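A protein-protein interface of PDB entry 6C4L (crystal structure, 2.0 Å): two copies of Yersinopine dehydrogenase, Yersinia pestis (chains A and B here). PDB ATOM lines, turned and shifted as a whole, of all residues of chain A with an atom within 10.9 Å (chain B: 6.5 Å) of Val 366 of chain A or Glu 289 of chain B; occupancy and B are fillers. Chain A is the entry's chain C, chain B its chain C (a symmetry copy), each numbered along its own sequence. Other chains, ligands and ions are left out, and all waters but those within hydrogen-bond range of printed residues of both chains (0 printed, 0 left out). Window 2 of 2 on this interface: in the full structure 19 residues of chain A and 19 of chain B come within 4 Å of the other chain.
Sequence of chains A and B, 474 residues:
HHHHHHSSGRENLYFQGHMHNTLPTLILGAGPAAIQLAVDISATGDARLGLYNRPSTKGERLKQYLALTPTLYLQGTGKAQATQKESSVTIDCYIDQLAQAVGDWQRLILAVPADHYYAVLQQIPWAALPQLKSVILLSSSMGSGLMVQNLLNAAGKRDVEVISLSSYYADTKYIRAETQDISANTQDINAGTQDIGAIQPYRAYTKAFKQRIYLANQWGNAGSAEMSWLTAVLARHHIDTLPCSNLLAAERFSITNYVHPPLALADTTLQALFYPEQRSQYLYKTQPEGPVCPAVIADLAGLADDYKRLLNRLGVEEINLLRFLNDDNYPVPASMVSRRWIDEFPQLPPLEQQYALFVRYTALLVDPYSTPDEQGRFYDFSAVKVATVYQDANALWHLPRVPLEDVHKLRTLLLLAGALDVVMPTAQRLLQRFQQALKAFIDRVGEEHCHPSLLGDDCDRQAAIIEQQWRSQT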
ATOM      1  N   TYR A 284      -3.097   8.363 -25.762  1.00  0.00           N
ATOM      2  CA  TYR A 284      -1.962   8.384 -24.850  1.00  0.00           C
ATOM      3  C   TYR A 284      -0.686   7.816 -25.466  1.00  0.00           C
ATOM      4  O   TYR A 284       0.365   7.834 -24.814  1.00  0.00           O
ATOM      5  CB  TYR A 284      -2.317   7.627 -23.551  1.00  0.00           C
ATOM      6  CG  TYR A 284      -3.391   8.313 -22.712  1.00  0.00           C
ATOM      7  CD1 TYR A 284      -3.067   9.317 -21.802  1.00  0.00           C
ATOM      8  CD2 TYR A 284      -4.735   7.970 -22.847  1.00  0.00           C
ATOM      9  CE1 TYR A 284      -4.059   9.969 -21.056  1.00  0.00           C
ATOM     10  CE2 TYR A 284      -5.734   8.617 -22.096  1.00  0.00           C
ATOM     11  CZ  TYR A 284      -5.383   9.612 -21.212  1.00  0.00           C
ATOM     12  OH  TYR A 284      -6.357  10.252 -20.486  1.00  0.00           O
ATOM     13  N   LYS A 285      -0.735   7.334 -26.699  1.00  0.00           N
ATOM     14  CA  LYS A 285       0.466   6.785 -27.318  1.00  0.00           C
ATOM     15  C   LYS A 285       1.362   7.881 -27.859  1.00  0.00           C
ATOM     16  O   LYS A 285       0.933   9.009 -28.099  1.00  0.00           O
ATOM     17  CB  LYS A 285       0.113   5.828 -28.440  1.00  0.00           C
ATOM     18  CG  LYS A 285      -0.400   4.499 -27.915  1.00  0.00           C
ATOM     19  CD  LYS A 285      -0.718   3.564 -29.041  1.00  0.00           C
ATOM     20  CE  LYS A 285      -1.534   2.396 -28.557  1.00  0.00           C
ATOM     21  NZ  LYS A 285      -1.963   1.553 -29.712  1.00  0.00           N
ATOM     22  N   THR A 286       2.633   7.525 -28.044  1.00  0.00           N
ATOM     23  CA  THR A 286       3.628   8.400 -28.642  1.00  0.00           C
ATOM     24  C   THR A 286       3.481   8.467 -30.160  1.00  0.00           C
ATOM     25  O   THR A 286       2.890   7.598 -30.812  1.00  0.00           O
ATOM     26  CB  THR A 286       5.047   7.926 -28.301  1.00  0.00           C
ATOM     27  OG1 THR A 286       5.092   6.499 -28.356  1.00  0.00           O
ATOM     28  CG2 THR A 286       5.468   8.392 -26.905  1.00  0.00           C
ATOM     29  N   TYR A 330      -2.619   7.388 -10.911  1.00  0.00           N
ATOM     30  CA  TYR A 330      -2.046   6.178 -11.514  1.00  0.00           C
ATOM     31  C   TYR A 330      -0.521   6.198 -11.389  1.00  0.00           C
ATOM     32  O   TYR A 330       0.132   7.018 -12.039  1.00  0.00           O
ATOM     33  CB  TYR A 330      -2.441   6.054 -12.989  1.00  0.00           C
ATOM     34  CG  TYR A 330      -3.918   6.298 -13.244  1.00  0.00           C
ATOM     35  CD1 TYR A 330      -4.870   5.306 -13.006  1.00  0.00           C
ATOM     36  CD2 TYR A 330      -4.365   7.532 -13.707  1.00  0.00           C
ATOM     37  CE1 TYR A 330      -6.231   5.541 -13.236  1.00  0.00           C
ATOM     38  CE2 TYR A 330      -5.721   7.777 -13.929  1.00  0.00           C
ATOM     39  CZ  TYR A 330      -6.643   6.777 -13.695  1.00  0.00           C
ATOM     40  OH  TYR A 330      -7.981   7.027 -13.919  1.00  0.00           O
ATOM     41  N   PRO A 331       0.077   5.346 -10.564  1.00  0.00           N
ATOM     42  CA  PRO A 331       1.514   5.459 -10.296  1.00  0.00           C
ATOM     43  C   PRO A 331       2.367   4.752 -11.329  1.00  0.00           C
ATOM     44  O   PRO A 331       1.945   3.822 -12.020  1.00  0.00           O
ATOM     45  CB  PRO A 331       1.663   4.781  -8.934  1.00  0.00           C
ATOM     46  CG  PRO A 331       0.641   3.738  -8.955  1.00  0.00           C
ATOM     47  CD  PRO A 331      -0.564   4.401  -9.623  1.00  0.00           C
ATOM     48  N   VAL A 332       3.602   5.223 -11.414  1.00  0.00           N
ATOM     49  CA  VAL A 332       4.601   4.527 -12.210  1.00  0.00           C
ATOM     50  C   VAL A 332       5.804   4.285 -11.312  1.00  0.00           C
ATOM     51  O   VAL A 332       6.009   4.983 -10.300  1.00  0.00           O
ATOM     52  CB  VAL A 332       4.965   5.322 -13.490  1.00  0.00           C
ATOM     53  CG1 VAL A 332       3.712   5.522 -14.352  1.00  0.00           C
ATOM     54  CG2 VAL A 332       5.612   6.644 -13.137  1.00  0.00           C
ATOM     55  N   PRO A 333       6.594   3.272 -11.635  1.00  0.00           N
ATOM     56  CA  PRO A 333       7.720   2.907 -10.769  1.00  0.00           C
ATOM     57  C   PRO A 333       8.675   4.076 -10.580  1.00  0.00           C
ATOM     58  O   PRO A 333       8.771   4.976 -11.415  1.00  0.00           O
ATOM     59  CB  PRO A 333       8.374   1.741 -11.511  1.00  0.00           C
ATOM     60  CG  PRO A 333       7.797   1.748 -12.891  1.00  0.00           C
ATOM     61  CD  PRO A 333       6.444   2.371 -12.784  1.00  0.00           C
ATOM     62  N   SER A 335      11.819   3.979 -10.565  1.00  0.00           N
ATOM     63  CA  SER A 335      12.940   3.893 -11.483  1.00  0.00           C
ATOM     64  C   SER A 335      12.677   4.678 -12.759  1.00  0.00           C
ATOM     65  O   SER A 335      13.621   4.966 -13.495  1.00  0.00           O
ATOM     66  CB  SER A 335      13.228   2.439 -11.845  1.00  0.00           C
ATOM     67  OG  SER A 335      12.157   1.927 -12.614  1.00  0.00           O
ATOM     68  N   MET A 336      11.415   5.002 -13.055  1.00  0.00           N
ATOM     69  CA  MET A 336      11.102   5.881 -14.178  1.00  0.00           C
ATOM     70  C   MET A 336      10.912   7.310 -13.694  1.00  0.00           C
ATOM     71  O   MET A 336      11.671   8.197 -14.089  1.00  0.00           O
ATOM     72  CB  MET A 336       9.865   5.386 -14.928  1.00  0.00           C
ATOM     73  CG  MET A 336      10.053   4.011 -15.545  1.00  0.00           C
ATOM     74  SD  MET A 336      11.189   4.069 -16.975  1.00  0.00           S
ATOM     75  CE  MET A 336      10.116   4.743 -18.233  1.00  0.00           C
ATOM     76  N   PHE A 358       7.176  13.576 -19.691  1.00  0.00           N
ATOM     77  CA  PHE A 358       7.323  12.652 -20.803  1.00  0.00           C
ATOM     78  C   PHE A 358       7.604  11.255 -20.297  1.00  0.00           C
ATOM     79  O   PHE A 358       7.013  10.281 -20.775  1.00  0.00           O
ATOM     80  CB  PHE A 358       8.439  13.095 -21.754  1.00  0.00           C
ATOM     81  CG  PHE A 358       8.546  12.225 -22.966  1.00  0.00           C
ATOM     82  CD1 PHE A 358       9.362  11.122 -22.968  1.00  0.00           C
ATOM     83  CD2 PHE A 358       7.793  12.502 -24.109  1.00  0.00           C
ATOM     84  CE1 PHE A 358       9.455  10.308 -24.102  1.00  0.00           C
ATOM     85  CE2 PHE A 358       7.883  11.708 -25.221  1.00  0.00           C
ATOM     86  CZ  PHE A 358       8.739  10.600 -25.212  1.00  0.00           C
ATOM     87  N   VAL A 359       8.509  11.136 -19.325  1.00  0.00           N
ATOM     88  CA  VAL A 359       8.830   9.822 -18.758  1.00  0.00           C
ATOM     89  C   VAL A 359       7.574   9.209 -18.148  1.00  0.00           C
ATOM     90  O   VAL A 359       7.236   8.043 -18.404  1.00  0.00           O
ATOM     91  CB  VAL A 359       9.976   9.943 -17.729  1.00  0.00           C
ATOM     92  CG1 VAL A 359      10.218   8.618 -16.989  1.00  0.00           C
ATOM     93  CG2 VAL A 359      11.325  10.360 -18.375  1.00  0.00           C
ATOM     94  N   ARG A 360       6.838  10.003 -17.365  1.00  0.00           N
ATOM     95  CA  ARG A 360       5.595   9.505 -16.780  1.00  0.00           C
ATOM     96  C   ARG A 360       4.687   8.893 -17.843  1.00  0.00           C
ATOM     97  O   ARG A 360       4.223   7.758 -17.696  1.00  0.00           O
ATOM     98  CB  ARG A 360       4.876  10.638 -16.055  1.00  0.00           C
ATOM     99  CG  ARG A 360       3.836  10.176 -15.060  1.00  0.00           C
ATOM    100  CD  ARG A 360       2.501  10.718 -15.384  1.00  0.00           C
ATOM    101  NE  ARG A 360       1.494  10.028 -14.603  1.00  0.00           N
ATOM    102  CZ  ARG A 360       0.194  10.050 -14.850  1.00  0.00           C
ATOM    103  NH1 ARG A 360      -0.291  10.739 -15.886  1.00  0.00           N
ATOM    104  NH2 ARG A 360      -0.623   9.370 -14.054  1.00  0.00           N
ATOM    105  N   TYR A 361       4.432   9.621 -18.942  1.00  0.00           N
ATOM    106  CA  TYR A 361       3.483   9.104 -19.926  1.00  0.00           C
ATOM    107  C   TYR A 361       4.055   7.948 -20.719  1.00  0.00           C
ATOM    108  O   TYR A 361       3.302   7.077 -21.173  1.00  0.00           O
ATOM    109  CB  TYR A 361       2.996  10.228 -20.848  1.00  0.00           C
ATOM    110  CG  TYR A 361       1.894  10.971 -20.143  1.00  0.00           C
ATOM    111  CD1 TYR A 361       0.620  10.424 -20.063  1.00  0.00           C
ATOM    112  CD2 TYR A 361       2.139  12.157 -19.471  1.00  0.00           C
ATOM    113  CE1 TYR A 361      -0.392  11.058 -19.374  1.00  0.00           C
ATOM    114  CE2 TYR A 361       1.124  12.797 -18.760  1.00  0.00           C
ATOM    115  CZ  TYR A 361      -0.138  12.241 -18.720  1.00  0.00           C
ATOM    116  OH  TYR A 361      -1.169  12.864 -18.030  1.00  0.00           O
ATOM    117  N   THR A 362       5.370   7.907 -20.897  1.00  0.00           N
ATOM    118  CA  THR A 362       5.972   6.711 -21.474  1.00  0.00           C
ATOM    119  C   THR A 362       5.782   5.515 -20.561  1.00  0.00           C
ATOM    120  O   THR A 362       5.405   4.432 -21.023  1.00  0.00           O
ATOM    121  CB  THR A 362       7.456   6.943 -21.751  1.00  0.00           C
ATOM    122  OG1 THR A 362       7.584   8.048 -22.639  1.00  0.00           O
ATOM    123  CG2 THR A 362       8.134   5.699 -22.400  1.00  0.00           C
ATOM    124  N   ALA A 363       6.033   5.693 -19.260  1.00  0.00           N
ATOM    125  CA  ALA A 363       5.932   4.582 -18.311  1.00  0.00           C
ATOM    126  C   ALA A 363       4.510   4.065 -18.185  1.00  0.00           C
ATOM    127  O   ALA A 363       4.304   2.864 -17.971  1.00  0.00           O
ATOM    128  CB  ALA A 363       6.423   5.006 -16.927  1.00  0.00           C
ATOM    129  N   LEU A 364       3.523   4.963 -18.308  1.00  0.00           N
ATOM    130  CA  LEU A 364       2.115   4.598 -18.199  1.00  0.00           C
ATOM    131  C   LEU A 364       1.708   3.578 -19.260  1.00  0.00           C
ATOM    132  O   LEU A 364       0.818   2.759 -19.020  1.00  0.00           O
ATOM    133  CB  LEU A 364       1.285   5.883 -18.312  1.00  0.00           C
ATOM    134  CG  LEU A 364       0.065   6.228 -17.458  1.00  0.00           C
ATOM    135  CD1 LEU A 364       0.301   6.134 -15.949  1.00  0.00           C
ATOM    136  CD2 LEU A 364      -0.397   7.654 -17.834  1.00  0.00           C
ATOM    137  N   LEU A 365       2.356   3.596 -20.430  1.00  0.00           N
ATOM    138  CA  LEU A 365       2.012   2.710 -21.540  1.00  0.00           C
ATOM    139  C   LEU A 365       2.595   1.307 -21.432  1.00  0.00           C
ATOM    140  O   LEU A 365       2.236   0.447 -22.246  1.00  0.00           O
ATOM    141  CB  LEU A 365       2.513   3.302 -22.862  1.00  0.00           C
ATOM    142  CG  LEU A 365       1.920   4.645 -23.273  1.00  0.00           C
ATOM    143  CD1 LEU A 365       2.649   5.191 -24.530  1.00  0.00           C
ATOM    144  CD2 LEU A 365       0.429   4.471 -23.512  1.00  0.00           C
ATOM    145  N   VAL A 366       3.506   1.070 -20.496  1.00  0.00           N
ATOM    146  CA  VAL A 366       4.182  -0.210 -20.370  1.00  0.00           C
ATOM    147  C   VAL A 366       3.553  -1.023 -19.239  1.00  0.00           C
ATOM    148  O   VAL A 366       2.335  -1.199 -19.191  1.00  0.00           O
ATOM    149  CB  VAL A 366       5.696   0.009 -20.135  1.00  0.00           C
ATOM    150  CG1 VAL A 366       6.388  -1.282 -19.765  1.00  0.00           C
ATOM    151  CG2 VAL A 366       6.328   0.626 -21.384  1.00  0.00           C
ATOM    152  N   TYR A 379      -4.951   0.142 -15.168  1.00  0.00           N
ATOM    153  CA  TYR A 379      -5.715   0.861 -16.187  1.00  0.00           C
ATOM    154  C   TYR A 379      -5.010   0.734 -17.540  1.00  0.00           C
ATOM    155  O   TYR A 379      -3.792   0.559 -17.589  1.00  0.00           O
ATOM    156  CB  TYR A 379      -5.889   2.337 -15.784  1.00  0.00           C
ATOM    157  CG  TYR A 379      -6.847   3.137 -16.656  1.00  0.00           C
ATOM    158  CD1 TYR A 379      -8.210   3.155 -16.398  1.00  0.00           C
ATOM    159  CD2 TYR A 379      -6.378   3.891 -17.721  1.00  0.00           C
ATOM    160  CE1 TYR A 379      -9.078   3.889 -17.190  1.00  0.00           C
ATOM    161  CE2 TYR A 379      -7.242   4.632 -18.518  1.00  0.00           C
ATOM    162  CZ  TYR A 379      -8.583   4.626 -18.249  1.00  0.00           C
ATOM    163  OH  TYR A 379      -9.412   5.368 -19.058  1.00  0.00           O
ATOM    164  N   ASP A 380      -5.772   0.817 -18.632  1.00  0.00           N
ATOM    165  CA  ASP A 380      -5.273   0.481 -19.969  1.00  0.00           C
ATOM    166  C   ASP A 380      -5.259   1.747 -20.826  1.00  0.00           C
ATOM    167  O   ASP A 380      -6.108   1.943 -21.702  1.00  0.00           O
ATOM    168  CB  ASP A 380      -6.142  -0.641 -20.610  1.00  0.00           C
ATOM    169  CG  ASP A 380      -5.376  -1.456 -21.639  1.00  0.00           C
ATOM    170  OD1 ASP A 380      -4.241  -1.063 -21.997  1.00  0.00           O
ATOM    171  OD2 ASP A 380      -5.910  -2.490 -22.092  1.00  0.00           O
ATOM    172  N   PHE A 381      -4.274   2.608 -20.573  1.00  0.00           N
ATOM    173  CA  PHE A 381      -4.143   3.825 -21.360  1.00  0.00           C
ATOM    174  C   PHE A 381      -3.901   3.506 -22.832  1.00  0.00           C
ATOM    175  O   PHE A 381      -4.470   4.155 -23.714  1.00  0.00           O
ATOM    176  CB  PHE A 381      -3.023   4.694 -20.791  1.00  0.00           C
ATOM    177  CG  PHE A 381      -3.387   5.358 -19.499  1.00  0.00           C
ATOM    178  CD1 PHE A 381      -4.122   6.524 -19.503  1.00  0.00           C
ATOM    179  CD2 PHE A 381      -3.018   4.802 -18.275  1.00  0.00           C
ATOM    180  CE1 PHE A 381      -4.483   7.144 -18.323  1.00  0.00           C
ATOM    181  CE2 PHE A 381      -3.375   5.427 -17.079  1.00  0.00           C
ATOM    182  CZ  PHE A 381      -4.107   6.597 -17.110  1.00  0.00           C
ATOM    183  N   SER A 382      -3.098   2.482 -23.112  1.00  0.00           N
ATOM    184  CA  SER A 382      -2.802   2.106 -24.490  1.00  0.00           C
ATOM    185  C   SER A 382      -4.051   1.841 -25.319  1.00  0.00           C
ATOM    186  O   SER A 382      -3.973   1.816 -26.550  1.00  0.00           O
ATOM    187  CB  SER A 382      -1.916   0.852 -24.499  1.00  0.00           C
ATOM    188  OG  SER A 382      -2.385  -0.094 -23.540  1.00  0.00           O
ATOM    189  N   ALA A 383      -5.186   1.618 -24.683  1.00  0.00           N
ATOM    190  CA  ALA A 383      -6.389   1.208 -25.386  1.00  0.00           C
ATOM    191  C   ALA A 383      -7.304   2.371 -25.760  1.00  0.00           C
ATOM    192  O   ALA A 383      -8.200   2.184 -26.594  1.00  0.00           O
ATOM    193  CB  ALA A 383      -7.175   0.216 -24.519  1.00  0.00           C
ATOM    194  N   SER B 280      12.787 -12.801 -18.699  1.00  0.00           N
ATOM    195  CA  SER B 280      13.684 -12.185 -19.657  1.00  0.00           C
ATOM    196  C   SER B 280      13.498 -10.673 -19.682  1.00  0.00           C
ATOM    197  O   SER B 280      12.402 -10.148 -19.470  1.00  0.00           O
ATOM    198  CB  SER B 280      13.442 -12.770 -21.045  1.00  0.00           C
ATOM    199  OG  SER B 280      13.655 -14.171 -21.032  1.00  0.00           O
ATOM    200  N   GLN B 281      14.602  -9.980 -19.902  1.00  0.00           N
ATOM    201  CA  GLN B 281      14.634  -8.551 -20.135  1.00  0.00           C
ATOM    202  C   GLN B 281      14.946  -8.301 -21.606  1.00  0.00           C
ATOM    203  O   GLN B 281      15.495  -9.159 -22.296  1.00  0.00           O
ATOM    204  CB  GLN B 281      15.689  -7.881 -19.250  1.00  0.00           C
ATOM    205  CG  GLN B 281      15.372  -7.871 -17.773  1.00  0.00           C
ATOM    206  CD  GLN B 281      14.385  -6.787 -17.431  1.00  0.00           C
ATOM    207  OE1 GLN B 281      14.735  -5.602 -17.393  1.00  0.00           O
ATOM    208  NE2 GLN B 281      13.135  -7.172 -17.225  1.00  0.00           N
ATOM    209  N   TYR B 282      14.564  -7.122 -22.087  1.00  0.00           N
ATOM    210  CA  TYR B 282      14.829  -6.695 -23.451  1.00  0.00           C
ATOM    211  C   TYR B 282      15.740  -5.486 -23.387  1.00  0.00           C
ATOM    212  O   TYR B 282      15.465  -4.535 -22.649  1.00  0.00           O
ATOM    213  CB  TYR B 282      13.528  -6.370 -24.207  1.00  0.00           C
ATOM    214  CG  TYR B 282      12.745  -7.627 -24.469  1.00  0.00           C
ATOM    215  CD1 TYR B 282      11.962  -8.186 -23.473  1.00  0.00           C
ATOM    216  CD2 TYR B 282      12.846  -8.300 -25.685  1.00  0.00           C
ATOM    217  CE1 TYR B 282      11.270  -9.353 -23.683  1.00  0.00           C
ATOM    218  CE2 TYR B 282      12.157  -9.479 -25.902  1.00  0.00           C
ATOM    219  CZ  TYR B 282      11.374  -9.999 -24.894  1.00  0.00           C
ATOM    220  OH  TYR B 282      10.674 -11.171 -25.083  1.00  0.00           O
ATOM    221  N   LEU B 283      16.810  -5.522 -24.174  1.00  0.00           N
ATOM    222  CA  LEU B 283      17.887  -4.563 -23.997  1.00  0.00           C
ATOM    223  C   LEU B 283      17.438  -3.124 -24.204  1.00  0.00           C
ATOM    224  O   LEU B 283      17.982  -2.218 -23.564  1.00  0.00           O
ATOM    225  CB  LEU B 283      19.024  -4.897 -24.956  1.00  0.00           C
ATOM    226  CG  LEU B 283      20.301  -4.114 -24.708  1.00  0.00           C
ATOM    227  CD1 LEU B 283      20.918  -4.493 -23.347  1.00  0.00           C
ATOM    228  CD2 LEU B 283      21.242  -4.353 -25.879  1.00  0.00           C
ATOM    229  N   LYS B 285      14.044  -1.948 -24.179  1.00  0.00           N
ATOM    230  CA  LYS B 285      12.753  -1.560 -23.623  1.00  0.00           C
ATOM    231  C   LYS B 285      12.918  -0.767 -22.341  1.00  0.00           C
ATOM    232  O   LYS B 285      13.953  -0.816 -21.678  1.00  0.00           O
ATOM    233  CB  LYS B 285      11.888  -2.775 -23.352  1.00  0.00           C
ATOM    234  CG  LYS B 285      11.322  -3.367 -24.630  1.00  0.00           C
ATOM    235  CD  LYS B 285      10.452  -4.550 -24.334  1.00  0.00           C
ATOM    236  CE  LYS B 285      10.171  -5.338 -25.586  1.00  0.00           C
ATOM    237  NZ  LYS B 285       9.425  -6.587 -25.251  1.00  0.00           N
ATOM    238  N   THR B 286      11.865  -0.024 -22.005  1.00  0.00           N
ATOM    239  CA  THR B 286      11.785   0.734 -20.766  1.00  0.00           C
ATOM    240  C   THR B 286      11.466  -0.165 -19.574  1.00  0.00           C
ATOM    241  O   THR B 286      10.944  -1.278 -19.700  1.00  0.00           O
ATOM    242  CB  THR B 286      10.715   1.829 -20.863  1.00  0.00           C
ATOM    243  OG1 THR B 286       9.582   1.318 -21.569  1.00  0.00           O
ATOM    244  CG2 THR B 286      11.249   3.065 -21.592  1.00  0.00           C
ATOM    245  N   GLN B 287      11.793   0.347 -18.398  1.00  0.00           N
ATOM    246  CA  GLN B 287      11.524  -0.376 -17.173  1.00  0.00           C
ATOM    247  C   GLN B 287      10.021  -0.614 -17.059  1.00  0.00           C
ATOM    248  O   GLN B 287       9.226   0.271 -17.410  1.00  0.00           O
ATOM    249  CB  GLN B 287      12.029   0.419 -15.976  1.00  0.00           C
ATOM    250  CG  GLN B 287      13.535   0.564 -15.923  1.00  0.00           C
ATOM    251  CD  GLN B 287      14.220  -0.678 -15.371  1.00  0.00           C
ATOM    252  OE1 GLN B 287      13.555  -1.564 -14.834  1.00  0.00           O
ATOM    253  NE2 GLN B 287      15.552  -0.754 -15.505  1.00  0.00           N
ATOM    254  N   PRO B 288       9.589  -1.790 -16.578  1.00  0.00           N
ATOM    255  CA  PRO B 288      10.375  -2.899 -16.021  1.00  0.00           C
ATOM    256  C   PRO B 288      10.720  -4.021 -16.993  1.00  0.00           C
ATOM    257  O   PRO B 288      11.186  -5.065 -16.544  1.00  0.00           O
ATOM    258  CB  PRO B 288       9.446  -3.439 -14.939  1.00  0.00           C
ATOM    259  CG  PRO B 288       8.098  -3.276 -15.558  1.00  0.00           C
ATOM    260  CD  PRO B 288       8.145  -2.026 -16.406  1.00  0.00           C
ATOM    261  N   GLU B 289      10.483  -3.825 -18.287  1.00  0.00           N
ATOM    262  CA  GLU B 289      10.766  -4.861 -19.271  1.00  0.00           C
ATOM    263  C   GLU B 289      12.183  -4.774 -19.826  1.00  0.00           C
ATOM    264  O   GLU B 289      12.679  -5.753 -20.397  1.00  0.00           O
ATOM    265  CB  GLU B 289       9.752  -4.779 -20.419  1.00  0.00           C
ATOM    266  CG  GLU B 289       8.320  -4.563 -19.949  1.00  0.00           C
ATOM    267  CD  GLU B 289       7.348  -4.554 -21.090  1.00  0.00           C
ATOM    268  OE1 GLU B 289       6.487  -5.460 -21.135  1.00  0.00           O
ATOM    269  OE2 GLU B 289       7.452  -3.645 -21.956  1.00  0.00           O
ATOM    270  N   GLY B 290      12.852  -3.645 -19.650  1.00  0.00           N
ATOM    271  CA  GLY B 290      14.239  -3.520 -20.004  1.00  0.00           C
ATOM    272  C   GLY B 290      14.822  -2.380 -19.213  1.00  0.00           C
ATOM    273  O   GLY B 290      14.185  -1.856 -18.296  1.00  0.00           O
ATOM    274  N   PRO B 291      16.020  -1.938 -19.573  1.00  0.00           N
ATOM    275  CA  PRO B 291      16.740  -1.019 -18.685  1.00  0.00           C
ATOM    276  C   PRO B 291      16.445   0.461 -18.902  1.00  0.00           C
ATOM    277  O   PRO B 291      16.747   1.260 -18.014  1.00  0.00           O
ATOM    278  CB  PRO B 291      18.209  -1.345 -18.987  1.00  0.00           C
ATOM    279  CG  PRO B 291      18.192  -1.759 -20.428  1.00  0.00           C
ATOM    280  CD  PRO B 291      16.862  -2.421 -20.684  1.00  0.00           C
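The backbone carbonyl oxygen (O) of Glu 289 of chain B lies within hydrogen-bond range of the backbone NH (N) of Tyr 282 of chain B.
The side-chain amide nitrogen (NE2) of Gln 287 of chain B sits close to the backbone carbonyl oxygen (O) of Pro 291 of chain B (3.4 Å).
The backbone carbonyl oxygen (O) of Pro 288 of chain B sits at hydrogen-bond distance from the side-chain amide nitrogen (NE2) of Gln 281 of chain B, at 2.9 Å.
O of Gly 290 of chain B sits close to NE2 of Gln 287 of chain B.
Pro 333 of chain A touches none of the printed residues of chain B.
Printed residues of chain B within 4 Å of Ser 335 of chain A: Gln 287 (3.7 Å).
Printed residues of chain B within 4 Å of Val 366 of chain A: Thr 286 (3.3 Å), Pro 288 (3.9 Å) and Glu 289 (3.4 Å).
Tyr 379 of chain A touches none of the printed residues of chain B.
No residue of chain A comes within 4 Å of Gln 281 of chain B.
No residue of chain A comes within 4 Å of Lys 285 of chain B.
Printed residues of chain A within 4 Å of Thr 286 of chain B: Met 336 and Val 366.
Of the printed residues of chain A, Gln 287 of chain B touches Ser 335 (3.7 Å) and Met 336 (3.9 Å).
Glu 289 of chain B touches one residue of chain A.
No residue of chain A comes within 4 Å of Gly 290 of chain B.
Among the printed residues, pairs that only touch across the chains: Ser 335 of chain A with Gln 287 of chain B, Met 336 of chain A with Thr 286 of chain B, Met 336 of chain A with Gln 287 of chain B, Val 366 of chain A with Thr 286 of chain B, Val 366 of chain A with Pro 288 of chain B and Val 366 of chain A with Glu 289 of chain B.
Of the 23 printed residues of chain A, 3 touch a printed residue of chain B.
Hydrophobic or aromatic side chains of chain A within 4 Å of the printed part of chain B: Met 336 and Val 366.
Along chain A the printed residues that touch a printed residue of chain B span positions 335 to 366.
Of the 11 printed residues of chain B, 4 touch a printed residue of chain A.
Along chain B the printed residues that touch a printed residue of chain A span positions 286 to 289.
Among the printed residues, 6 pairs touch across the chains.
2 positions are printed for both chains.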
